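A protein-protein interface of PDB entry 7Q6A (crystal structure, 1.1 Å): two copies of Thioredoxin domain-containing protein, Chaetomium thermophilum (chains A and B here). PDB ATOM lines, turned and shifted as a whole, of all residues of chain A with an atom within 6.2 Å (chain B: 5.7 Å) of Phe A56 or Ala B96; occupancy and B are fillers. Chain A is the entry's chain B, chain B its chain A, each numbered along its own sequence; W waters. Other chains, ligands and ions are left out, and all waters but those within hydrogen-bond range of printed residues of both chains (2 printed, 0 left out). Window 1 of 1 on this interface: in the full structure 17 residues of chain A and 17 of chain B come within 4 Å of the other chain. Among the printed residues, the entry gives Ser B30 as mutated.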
ATOM      1  N   LEU A  27     -11.285  28.665  10.294  1.00  0.00           N
ATOM      2  CA  LEU A  27     -10.023  28.096  10.720  1.00  0.00           C
ATOM      3  C   LEU A  27      -9.905  28.031  12.236  1.00  0.00           C
ATOM      4  O   LEU A  27      -8.975  27.369  12.715  1.00  0.00           O
ATOM      5  CB  LEU A  27      -8.844  28.874  10.113  1.00  0.00           C
ATOM      6  CG  LEU A  27      -8.451  28.534   8.678  1.00  0.00           C
ATOM      7  CD1 LEU A  27      -9.449  29.082   7.683  1.00  0.00           C
ATOM      8  CD2 LEU A  27      -7.069  29.045   8.363  1.00  0.00           C
ATOM      9  N   GLY A  54       5.443  21.833   2.573  1.00  0.00           N
ATOM     10  CA  GLY A  54       4.833  22.441   3.741  1.00  0.00           C
ATOM     11  C   GLY A  54       3.566  23.220   3.495  1.00  0.00           C
ATOM     12  O   GLY A  54       3.536  24.112   2.637  1.00  0.00           O
ATOM     13  N   ALA A  55       2.535  22.925   4.283  1.00  0.00           N
ATOM     14  CA  ALA A  55       1.339  23.759   4.278  1.00  0.00           C
ATOM     15  C   ALA A  55       1.745  25.214   4.488  1.00  0.00           C
ATOM     16  O   ALA A  55       2.629  25.530   5.307  1.00  0.00           O
ATOM     17  CB  ALA A  55       0.424  23.337   5.421  1.00  0.00           C
ATOM     18  N   PHE A  56       1.091  26.113   3.757  1.00  0.00           N
ATOM     19  CA  PHE A  56       1.254  27.561   3.853  1.00  0.00           C
ATOM     20  C   PHE A  56       2.596  28.084   3.354  1.00  0.00           C
ATOM     21  O   PHE A  56       2.796  29.303   3.367  1.00  0.00           O
ATOM     22  CB  PHE A  56       0.981  28.111   5.266  1.00  0.00           C
ATOM     23  CG  PHE A  56      -0.455  27.949   5.726  1.00  0.00           C
ATOM     24  CD1 PHE A  56      -1.444  28.807   5.275  1.00  0.00           C
ATOM     25  CD2 PHE A  56      -0.801  26.968   6.634  1.00  0.00           C
ATOM     26  CE1 PHE A  56      -2.755  28.662   5.700  1.00  0.00           C
ATOM     27  CE2 PHE A  56      -2.112  26.837   7.075  1.00  0.00           C
ATOM     28  CZ  PHE A  56      -3.076  27.692   6.599  1.00  0.00           C
ATOM     29  N   THR A  57       3.492  27.240   2.884  1.00  0.00           N
ATOM     30  CA  THR A  57       4.769  27.772   2.408  1.00  0.00           C
ATOM     31  C   THR A  57       4.650  28.256   0.954  1.00  0.00           C
ATOM     32  O   THR A  57       3.665  27.935   0.269  1.00  0.00           O
ATOM     33  CB  THR A  57       5.887  26.746   2.581  1.00  0.00           C
ATOM     34  OG1 THR A  57       5.731  25.657   1.661  1.00  0.00           O
ATOM     35  CG2 THR A  57       5.949  26.227   4.012  1.00  0.00           C
ATOM     36  N   PRO A  58       5.590  29.075   0.487  1.00  0.00           N
ATOM     37  CA  PRO A  58       5.322  29.875  -0.741  1.00  0.00           C
ATOM     38  C   PRO A  58       4.959  29.077  -1.975  1.00  0.00           C
ATOM     39  O   PRO A  58       3.942  29.383  -2.618  1.00  0.00           O
ATOM     40  CB  PRO A  58       6.610  30.687  -0.906  1.00  0.00           C
ATOM     41  CG  PRO A  58       7.072  30.889   0.516  1.00  0.00           C
ATOM     42  CD  PRO A  58       6.771  29.574   1.212  1.00  0.00           C
ATOM     43  N   CYS A  60       4.187  25.825  -2.281  1.00  0.00           N
ATOM     44  CA  CYS A  60       3.083  24.917  -1.999  1.00  0.00           C
ATOM     45  C   CYS A  60       1.746  25.631  -2.058  1.00  0.00           C
ATOM     46  O   CYS A  60       0.766  25.099  -2.613  1.00  0.00           O
ATOM     47  CB  CYS A  60       3.301  24.299  -0.620  1.00  0.00           C
ATOM     48  SG  CYS A  60       4.912  23.472  -0.453  1.00  0.00           S
ATOM     49  N   GLN A  61       1.659  26.813  -1.445  1.00  0.00           N
ATOM     50  CA  GLN A  61       0.432  27.584  -1.417  1.00  0.00           C
ATOM     51  C   GLN A  61       0.201  28.329  -2.720  1.00  0.00           C
ATOM     52  O   GLN A  61      -0.863  28.205  -3.333  1.00  0.00           O
ATOM     53  CB  GLN A  61       0.483  28.591  -0.259  1.00  0.00           C
ATOM     54  CG  GLN A  61      -0.620  29.627  -0.275  1.00  0.00           C
ATOM     55  CD  GLN A  61      -2.006  29.004  -0.265  1.00  0.00           C
ATOM     56  OE1 GLN A  61      -2.257  28.079   0.520  1.00  0.00           O
ATOM     57  NE2 GLN A  61      -2.908  29.485  -1.087  1.00  0.00           N
ATOM     58  N   ASN A  89       3.090  18.327   7.964  1.00  0.00           N
ATOM     59  CA  ASN A  89       2.322  19.069   8.947  1.00  0.00           C
ATOM     60  C   ASN A  89       1.222  18.181   9.515  1.00  0.00           C
ATOM     61  O   ASN A  89       0.664  17.338   8.798  1.00  0.00           O
ATOM     62  CB  ASN A  89       1.664  20.290   8.289  1.00  0.00           C
ATOM     63  CG  ASN A  89       2.618  21.152   7.493  1.00  0.00           C
ATOM     64  OD1 ASN A  89       2.908  20.865   6.331  1.00  0.00           O
ATOM     65  ND2 ASN A  89       3.131  22.215   8.115  1.00  0.00           N
ATOM     66  N   VAL A  93      -3.123  21.457  11.198  1.00  0.00           N
ATOM     67  CA  VAL A  93      -2.570  22.413  10.242  1.00  0.00           C
ATOM     68  C   VAL A  93      -3.059  22.109   8.836  1.00  0.00           C
ATOM     69  O   VAL A  93      -3.402  23.025   8.087  1.00  0.00           O
ATOM     70  CB  VAL A  93      -1.033  22.453  10.340  1.00  0.00           C
ATOM     71  CG1 VAL A  93      -0.432  23.332   9.300  1.00  0.00           C
ATOM     72  CG2 VAL A  93      -0.630  22.853  11.758  1.00  0.00           C
ATOM     73  N   ALA A  96      -6.625  23.307   8.434  1.00  0.00           N
ATOM     74  CA  ALA A  96      -6.632  24.767   8.319  1.00  0.00           C
ATOM     75  C   ALA A  96      -6.177  25.215   6.943  1.00  0.00           C
ATOM     76  O   ALA A  96      -6.758  26.132   6.352  1.00  0.00           O
ATOM     77  CB  ALA A  96      -5.748  25.374   9.403  1.00  0.00           C
ATOM     78  N   TRP A  97      -5.163  24.554   6.394  1.00  0.00           N
ATOM     79  CA  TRP A  97      -4.656  24.906   5.077  1.00  0.00           C
ATOM     80  C   TRP A  97      -5.714  24.664   3.999  1.00  0.00           C
ATOM     81  O   TRP A  97      -5.909  25.503   3.112  1.00  0.00           O
ATOM     82  CB  TRP A  97      -3.368  24.116   4.824  1.00  0.00           C
ATOM     83  CG  TRP A  97      -2.637  24.567   3.605  1.00  0.00           C
ATOM     84  CD1 TRP A  97      -2.403  25.859   3.218  1.00  0.00           C
ATOM     85  CD2 TRP A  97      -2.012  23.738   2.601  1.00  0.00           C
ATOM     86  NE1 TRP A  97      -1.659  25.882   2.052  1.00  0.00           N
ATOM     87  CE2 TRP A  97      -1.448  24.595   1.635  1.00  0.00           C
ATOM     88  CE3 TRP A  97      -1.887  22.361   2.431  1.00  0.00           C
ATOM     89  CZ2 TRP A  97      -0.779  24.106   0.510  1.00  0.00           C
ATOM     90  CZ3 TRP A  97      -1.245  21.882   1.323  1.00  0.00           C
ATOM     91  CH2 TRP A  97      -0.698  22.753   0.369  1.00  0.00           C
ATOM     92  N   GLY A  98      -6.434  23.547   4.083  1.00  0.00           N
ATOM     93  CA  GLY A  98      -7.525  23.304   3.155  1.00  0.00           C
ATOM     94  C   GLY A  98      -8.593  24.369   3.250  1.00  0.00           C
ATOM     95  O   GLY A  98      -9.076  24.889   2.235  1.00  0.00           O
ATOM     96  N   ALA A 100      -8.252  27.410   4.362  1.00  0.00           N
ATOM     97  CA  ALA A 100      -7.721  28.681   3.885  1.00  0.00           C
ATOM     98  C   ALA A 100      -7.853  28.803   2.374  1.00  0.00           C
ATOM     99  O   ALA A 100      -7.894  29.919   1.827  1.00  0.00           O
ATOM    100  CB  ALA A 100      -6.244  28.842   4.278  1.00  0.00           C
ATOM    101  N   ASN A 101      -7.869  27.664   1.686  1.00  0.00           N
ATOM    102  CA  ASN A 101      -8.032  27.600   0.244  1.00  0.00           C
ATOM    103  C   ASN A 101      -9.463  27.355  -0.180  1.00  0.00           C
ATOM    104  O   ASN A 101      -9.696  27.072  -1.358  1.00  0.00           O
ATOM    105  CB  ASN A 101      -7.090  26.555  -0.307  1.00  0.00           C
ATOM    106  CG  ASN A 101      -5.669  27.073  -0.340  1.00  0.00           C
ATOM    107  OD1 ASN A 101      -5.342  27.891  -1.184  1.00  0.00           O
ATOM    108  ND2 ASN A 101      -4.839  26.659   0.592  1.00  0.00           N
ATOM    109  N   LEU B  27      -4.868  34.827   3.983  1.00  0.00           N
ATOM    110  CA  LEU B  27      -4.161  33.600   4.323  1.00  0.00           C
ATOM    111  C   LEU B  27      -3.435  32.998   3.135  1.00  0.00           C
ATOM    112  O   LEU B  27      -2.576  32.119   3.323  1.00  0.00           O
ATOM    113  CB  LEU B  27      -5.162  32.568   4.831  1.00  0.00           C
ATOM    114  CG  LEU B  27      -5.700  32.846   6.222  1.00  0.00           C
ATOM    115  CD1 LEU B  27      -7.036  32.196   6.412  1.00  0.00           C
ATOM    116  CD2 LEU B  27      -4.721  32.314   7.247  1.00  0.00           C
ATOM    117  N   SER B  30       1.817  33.856   1.475  1.00  0.00           N
ATOM    118  CA  SER B  30       2.663  33.113   2.404  1.00  0.00           C
ATOM    119  C   SER B  30       3.478  34.038   3.292  1.00  0.00           C
ATOM    120  O   SER B  30       3.585  33.801   4.497  1.00  0.00           O
ATOM    121  CB  SER B  30       3.569  32.144   1.646  1.00  0.00           C
ATOM    122  OG  SER B  30       2.794  31.124   1.041  1.00  0.00           O
ATOM    123  N   PHE B  56      -3.089  25.843  15.703  1.00  0.00           N
ATOM    124  CA  PHE B  56      -4.317  25.251  15.189  1.00  0.00           C
ATOM    125  C   PHE B  56      -4.777  24.020  15.966  1.00  0.00           C
ATOM    126  O   PHE B  56      -5.794  23.439  15.602  1.00  0.00           O
ATOM    127  CB  PHE B  56      -4.256  24.931  13.683  1.00  0.00           C
ATOM    128  CG  PHE B  56      -4.121  26.150  12.810  1.00  0.00           C
ATOM    129  CD1 PHE B  56      -5.212  26.972  12.563  1.00  0.00           C
ATOM    130  CD2 PHE B  56      -2.913  26.470  12.187  1.00  0.00           C
ATOM    131  CE1 PHE B  56      -5.087  28.076  11.760  1.00  0.00           C
ATOM    132  CE2 PHE B  56      -2.783  27.587  11.390  1.00  0.00           C
ATOM    133  CZ  PHE B  56      -3.870  28.376  11.161  1.00  0.00           C
ATOM    134  N   ALA B  91       7.479  29.464  10.518  1.00  0.00           N
ATOM    135  CA  ALA B  91       6.997  30.835  10.505  1.00  0.00           C
ATOM    136  C   ALA B  91       5.785  31.011   9.602  1.00  0.00           C
ATOM    137  O   ALA B  91       4.951  31.908   9.846  1.00  0.00           O
ATOM    138  CB  ALA B  91       8.119  31.749  10.048  1.00  0.00           C
ATOM    139  N   PHE B  92       5.708  30.260   8.510  1.00  0.00           N
ATOM    140  CA  PHE B  92       4.553  30.402   7.619  1.00  0.00           C
ATOM    141  C   PHE B  92       3.268  29.950   8.305  1.00  0.00           C
ATOM    142  O   PHE B  92       2.230  30.610   8.192  1.00  0.00           O
ATOM    143  CB  PHE B  92       4.790  29.597   6.356  1.00  0.00           C
ATOM    144  CG  PHE B  92       5.970  30.051   5.572  1.00  0.00           C
ATOM    145  CD1 PHE B  92       5.919  31.178   4.763  1.00  0.00           C
ATOM    146  CD2 PHE B  92       7.173  29.379   5.641  1.00  0.00           C
ATOM    147  CE1 PHE B  92       7.022  31.608   4.045  1.00  0.00           C
ATOM    148  CE2 PHE B  92       8.281  29.804   4.917  1.00  0.00           C
ATOM    149  CZ  PHE B  92       8.198  30.918   4.134  1.00  0.00           C
ATOM    150  N   VAL B  93       3.309  28.817   8.994  1.00  0.00           N
ATOM    151  CA  VAL B  93       2.158  28.320   9.726  1.00  0.00           C
ATOM    152  C   VAL B  93       1.797  29.259  10.865  1.00  0.00           C
ATOM    153  O   VAL B  93       0.612  29.539  11.095  1.00  0.00           O
ATOM    154  CB  VAL B  93       2.419  26.880  10.209  1.00  0.00           C
ATOM    155  CG1 VAL B  93       1.312  26.377  11.109  1.00  0.00           C
ATOM    156  CG2 VAL B  93       2.648  25.944   9.033  1.00  0.00           C
ATOM    157  N   MET B  94       2.805  29.768  11.588  1.00  0.00           N
ATOM    158  CA  MET B  94       2.524  30.686  12.683  1.00  0.00           C
ATOM    159  C   MET B  94       1.876  31.979  12.192  1.00  0.00           C
ATOM    160  O   MET B  94       0.961  32.526  12.830  1.00  0.00           O
ATOM    161  CB  MET B  94       3.801  30.989  13.463  1.00  0.00           C
ATOM    162  CG  MET B  94       4.338  29.796  14.259  1.00  0.00           C
ATOM    163  SD  MET B  94       3.196  29.088  15.450  1.00  0.00           S
ATOM    164  CE  MET B  94       3.168  30.375  16.716  1.00  0.00           C
ATOM    165  N   SER B  95       2.349  32.488  11.059  1.00  0.00           N
ATOM    166  CA  SER B  95       1.746  33.687  10.473  1.00  0.00           C
ATOM    167  C   SER B  95       0.297  33.438  10.107  1.00  0.00           C
ATOM    168  O   SER B  95      -0.573  34.257  10.428  1.00  0.00           O
ATOM    169  CB  SER B  95       2.577  34.085   9.262  1.00  0.00           C
ATOM    170  OG  SER B  95       2.027  35.205   8.564  1.00  0.00           O
ATOM    171  N   ALA B  96       0.015  32.305   9.477  1.00  0.00           N
ATOM    172  CA  ALA B  96      -1.354  31.933   9.161  1.00  0.00           C
ATOM    173  C   ALA B  96      -2.211  31.830  10.410  1.00  0.00           C
ATOM    174  O   ALA B  96      -3.391  32.203  10.405  1.00  0.00           O
ATOM    175  CB  ALA B  96      -1.370  30.606   8.402  1.00  0.00           C
ATOM    176  N   TRP B  97      -1.662  31.270  11.488  1.00  0.00           N
ATOM    177  CA  TRP B  97      -2.412  31.109  12.727  1.00  0.00           C
ATOM    178  C   TRP B  97      -2.817  32.468  13.286  1.00  0.00           C
ATOM    179  O   TRP B  97      -3.957  32.676  13.703  1.00  0.00           O
ATOM    180  CB  TRP B  97      -1.579  30.291  13.712  1.00  0.00           C
ATOM    181  CG  TRP B  97      -2.340  29.823  14.892  1.00  0.00           C
ATOM    182  CD1 TRP B  97      -3.630  29.350  14.939  1.00  0.00           C
ATOM    183  CD2 TRP B  97      -1.860  29.776  16.248  1.00  0.00           C
ATOM    184  NE1 TRP B  97      -3.956  28.992  16.232  1.00  0.00           N
ATOM    185  CE2 TRP B  97      -2.891  29.269  17.052  1.00  0.00           C
ATOM    186  CE3 TRP B  97      -0.634  30.093  16.851  1.00  0.00           C
ATOM    187  CZ2 TRP B  97      -2.751  29.100  18.433  1.00  0.00           C
ATOM    188  CZ3 TRP B  97      -0.517  29.950  18.211  1.00  0.00           C
ATOM    189  CH2 TRP B  97      -1.552  29.470  18.979  1.00  0.00           C
ATOM    190  N   GLY B  98      -1.906  33.433  13.248  1.00  0.00           N
ATOM    191  CA  GLY B  98      -2.250  34.766  13.691  1.00  0.00           C
ATOM    192  C   GLY B  98      -3.324  35.397  12.827  1.00  0.00           C
ATOM    193  O   GLY B  98      -4.236  36.027  13.344  1.00  0.00           O
ATOM    194  N   LYS B  99      -3.218  35.256  11.496  1.00  0.00           N
ATOM    195  CA  LYS B  99      -4.233  35.783  10.594  1.00  0.00           C
ATOM    196  C   LYS B  99      -5.586  35.136  10.837  1.00  0.00           C
ATOM    197  O   LYS B  99      -6.615  35.813  10.804  1.00  0.00           O
ATOM    198  CB  LYS B  99      -3.835  35.561   9.137  1.00  0.00           C
ATOM    199  CG  LYS B  99      -2.619  36.323   8.666  1.00  0.00           C
ATOM    200  CD  LYS B  99      -2.243  35.861   7.271  1.00  0.00           C
ATOM    201  CE  LYS B  99      -0.845  36.240   6.863  1.00  0.00           C
ATOM    202  NZ  LYS B  99      -0.526  35.627   5.552  1.00  0.00           N
ATOM    203  N   ALA B 100      -5.600  33.822  11.084  1.00  0.00           N
ATOM    204  CA  ALA B 100      -6.853  33.130  11.330  1.00  0.00           C
ATOM    205  C   ALA B 100      -7.545  33.679  12.562  1.00  0.00           C
ATOM    206  O   ALA B 100      -8.779  33.642  12.658  1.00  0.00           O
ATOM    207  CB  ALA B 100      -6.596  31.638  11.494  1.00  0.00           C
ATOM    208  N   ASN B 101      -6.767  34.211  13.498  1.00  0.00           N
ATOM    209  CA  ASN B 101      -7.277  34.803  14.716  1.00  0.00           C
ATOM    210  C   ASN B 101      -7.478  36.301  14.612  1.00  0.00           C
ATOM    211  O   ASN B 101      -7.766  36.947  15.631  1.00  0.00           O
ATOM    212  CB  ASN B 101      -6.370  34.448  15.882  1.00  0.00           C
ATOM    213  CG  ASN B 101      -6.613  33.046  16.358  1.00  0.00           C
ATOM    214  OD1 ASN B 101      -7.593  32.790  17.020  1.00  0.00           O
ATOM    215  ND2 ASN B 101      -5.741  32.122  16.007  1.00  0.00           N
HETATM  216  O   HOH W   1      -7.883  25.652  14.664  1.00  0.00           O
HETATM  217  O   HOH W   2       0.078  30.810   2.694  1.00  0.00           O
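Leu B27 touches Leu A27.
Phe B56 touches Leu A27 (CD1 to O, 3.8 Å).
CB of Leu A27 touches CB of Ala B100, at 3.8 Å.
O of Phe A56 touches CB of Phe B92, 3.6 Å away.
Phe B92 touches Thr A57 (CD2 to CG2, 3.8 Å).
OG of Ser B30 touches CA of Pro A58, at 3.3 Å.
Gln A61 touches Ser B30 (CB to OG, 3.7 Å).
Asn A89 touches Val B93.
Ala A96 touches Phe B56.
Leu B27 touches Ala A100.
The side-chain hydroxyl of Thr A57 sits at hydrogen-bond distance from the backbone carbonyl oxygen of Gly A54 (2.9 Å).
The side-chain sulfur (SG) of Cys A60 is in hydrogen-bond range of the side-chain hydroxyl (OG1) of Thr A57, at 3.1 Å.
The backbone NH of Ala A55 sits at hydrogen-bond distance from the side-chain amide oxygen of Asn A89.
OD1 of Asn A101 is in hydrogen-bond range of NE2 of Gln A61 (2.9 Å).
The side-chain amide oxygen of Gln A61 lies within hydrogen-bond range of the indole nitrogen of Trp A97, 2.7 Å away.
The side-chain hydroxyl of Ser B30 is in hydrogen-bond range of the backbone carbonyl oxygen of Phe A56 (3.0 Å).
The side-chain hydroxyl (OG) of Ser B30 is in hydrogen-bond range of the backbone carbonyl oxygen (O) of Thr A57, 3.4 Å away.
Leu A27 touches its own counterpart, Leu B27.
Leu A27 touches Phe B56, but with the chains exchanged Phe A56 does not touch Leu B27 (4.01 Å).
Leu A27 touches Ala B100, and with the chains exchanged Ala A100 touches Leu B27.
Phe A56 touches Ala B96, and with the chains exchanged Ala A96 touches Phe B56.
Positions printed for both chains: 27, 56, 93, 96, 97, 98, 100 and 101.
Hydrophobic or aromatic side chains of chain B within 4 Å of the printed part of chain A: Leu B27, Phe B56, Phe B92, Val B93, Ala B96 and Ala B100.
Along chain B the printed residues that touch a printed residue of chain A span positions 27 to 100.
Among the printed residues, no Asp or Glu carboxylate lies within 4 Å of a Lys or Arg side-chain nitrogen of the other chain.
Water W1 bridges the backbone carbonyl oxygen of Leu A27 (2.8 Å) and the backbone carbonyl oxygen of Phe B56 (3.2 Å).
Water W2 lies within hydrogen-bond range of the backbone carbonyl oxygen of Leu B27, the backbone carbonyl oxygen of Phe A56 and the side-chain hydroxyl of Ser B30.
Printed residues of chain B within 4 Å of Leu A27: Leu B27 (3.7 Å), Phe B56 (3.8 Å) and Ala B100 (3.8 Å).
Of the printed residues of chain B, Phe A56 touches Ser B30, Phe B92 and Ala B96.
Printed residues of chain B within 4 Å of Gln A61: Ser B30.
Of the printed residues of chain A, Ser B30 touches Phe A56 (3.0 Å), Thr A57 (3.4 Å), Pro A58 (3.3 Å) and Gln A61 (3.7 Å).
Of the printed residues of chain A, Val B93 touches Ala A55, Asn A89 and Val A93.
Ala B96 touches just one residue of chain A: Phe A56.
Printed residues of chain A within 4 Å of Ala B100: Leu A27.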
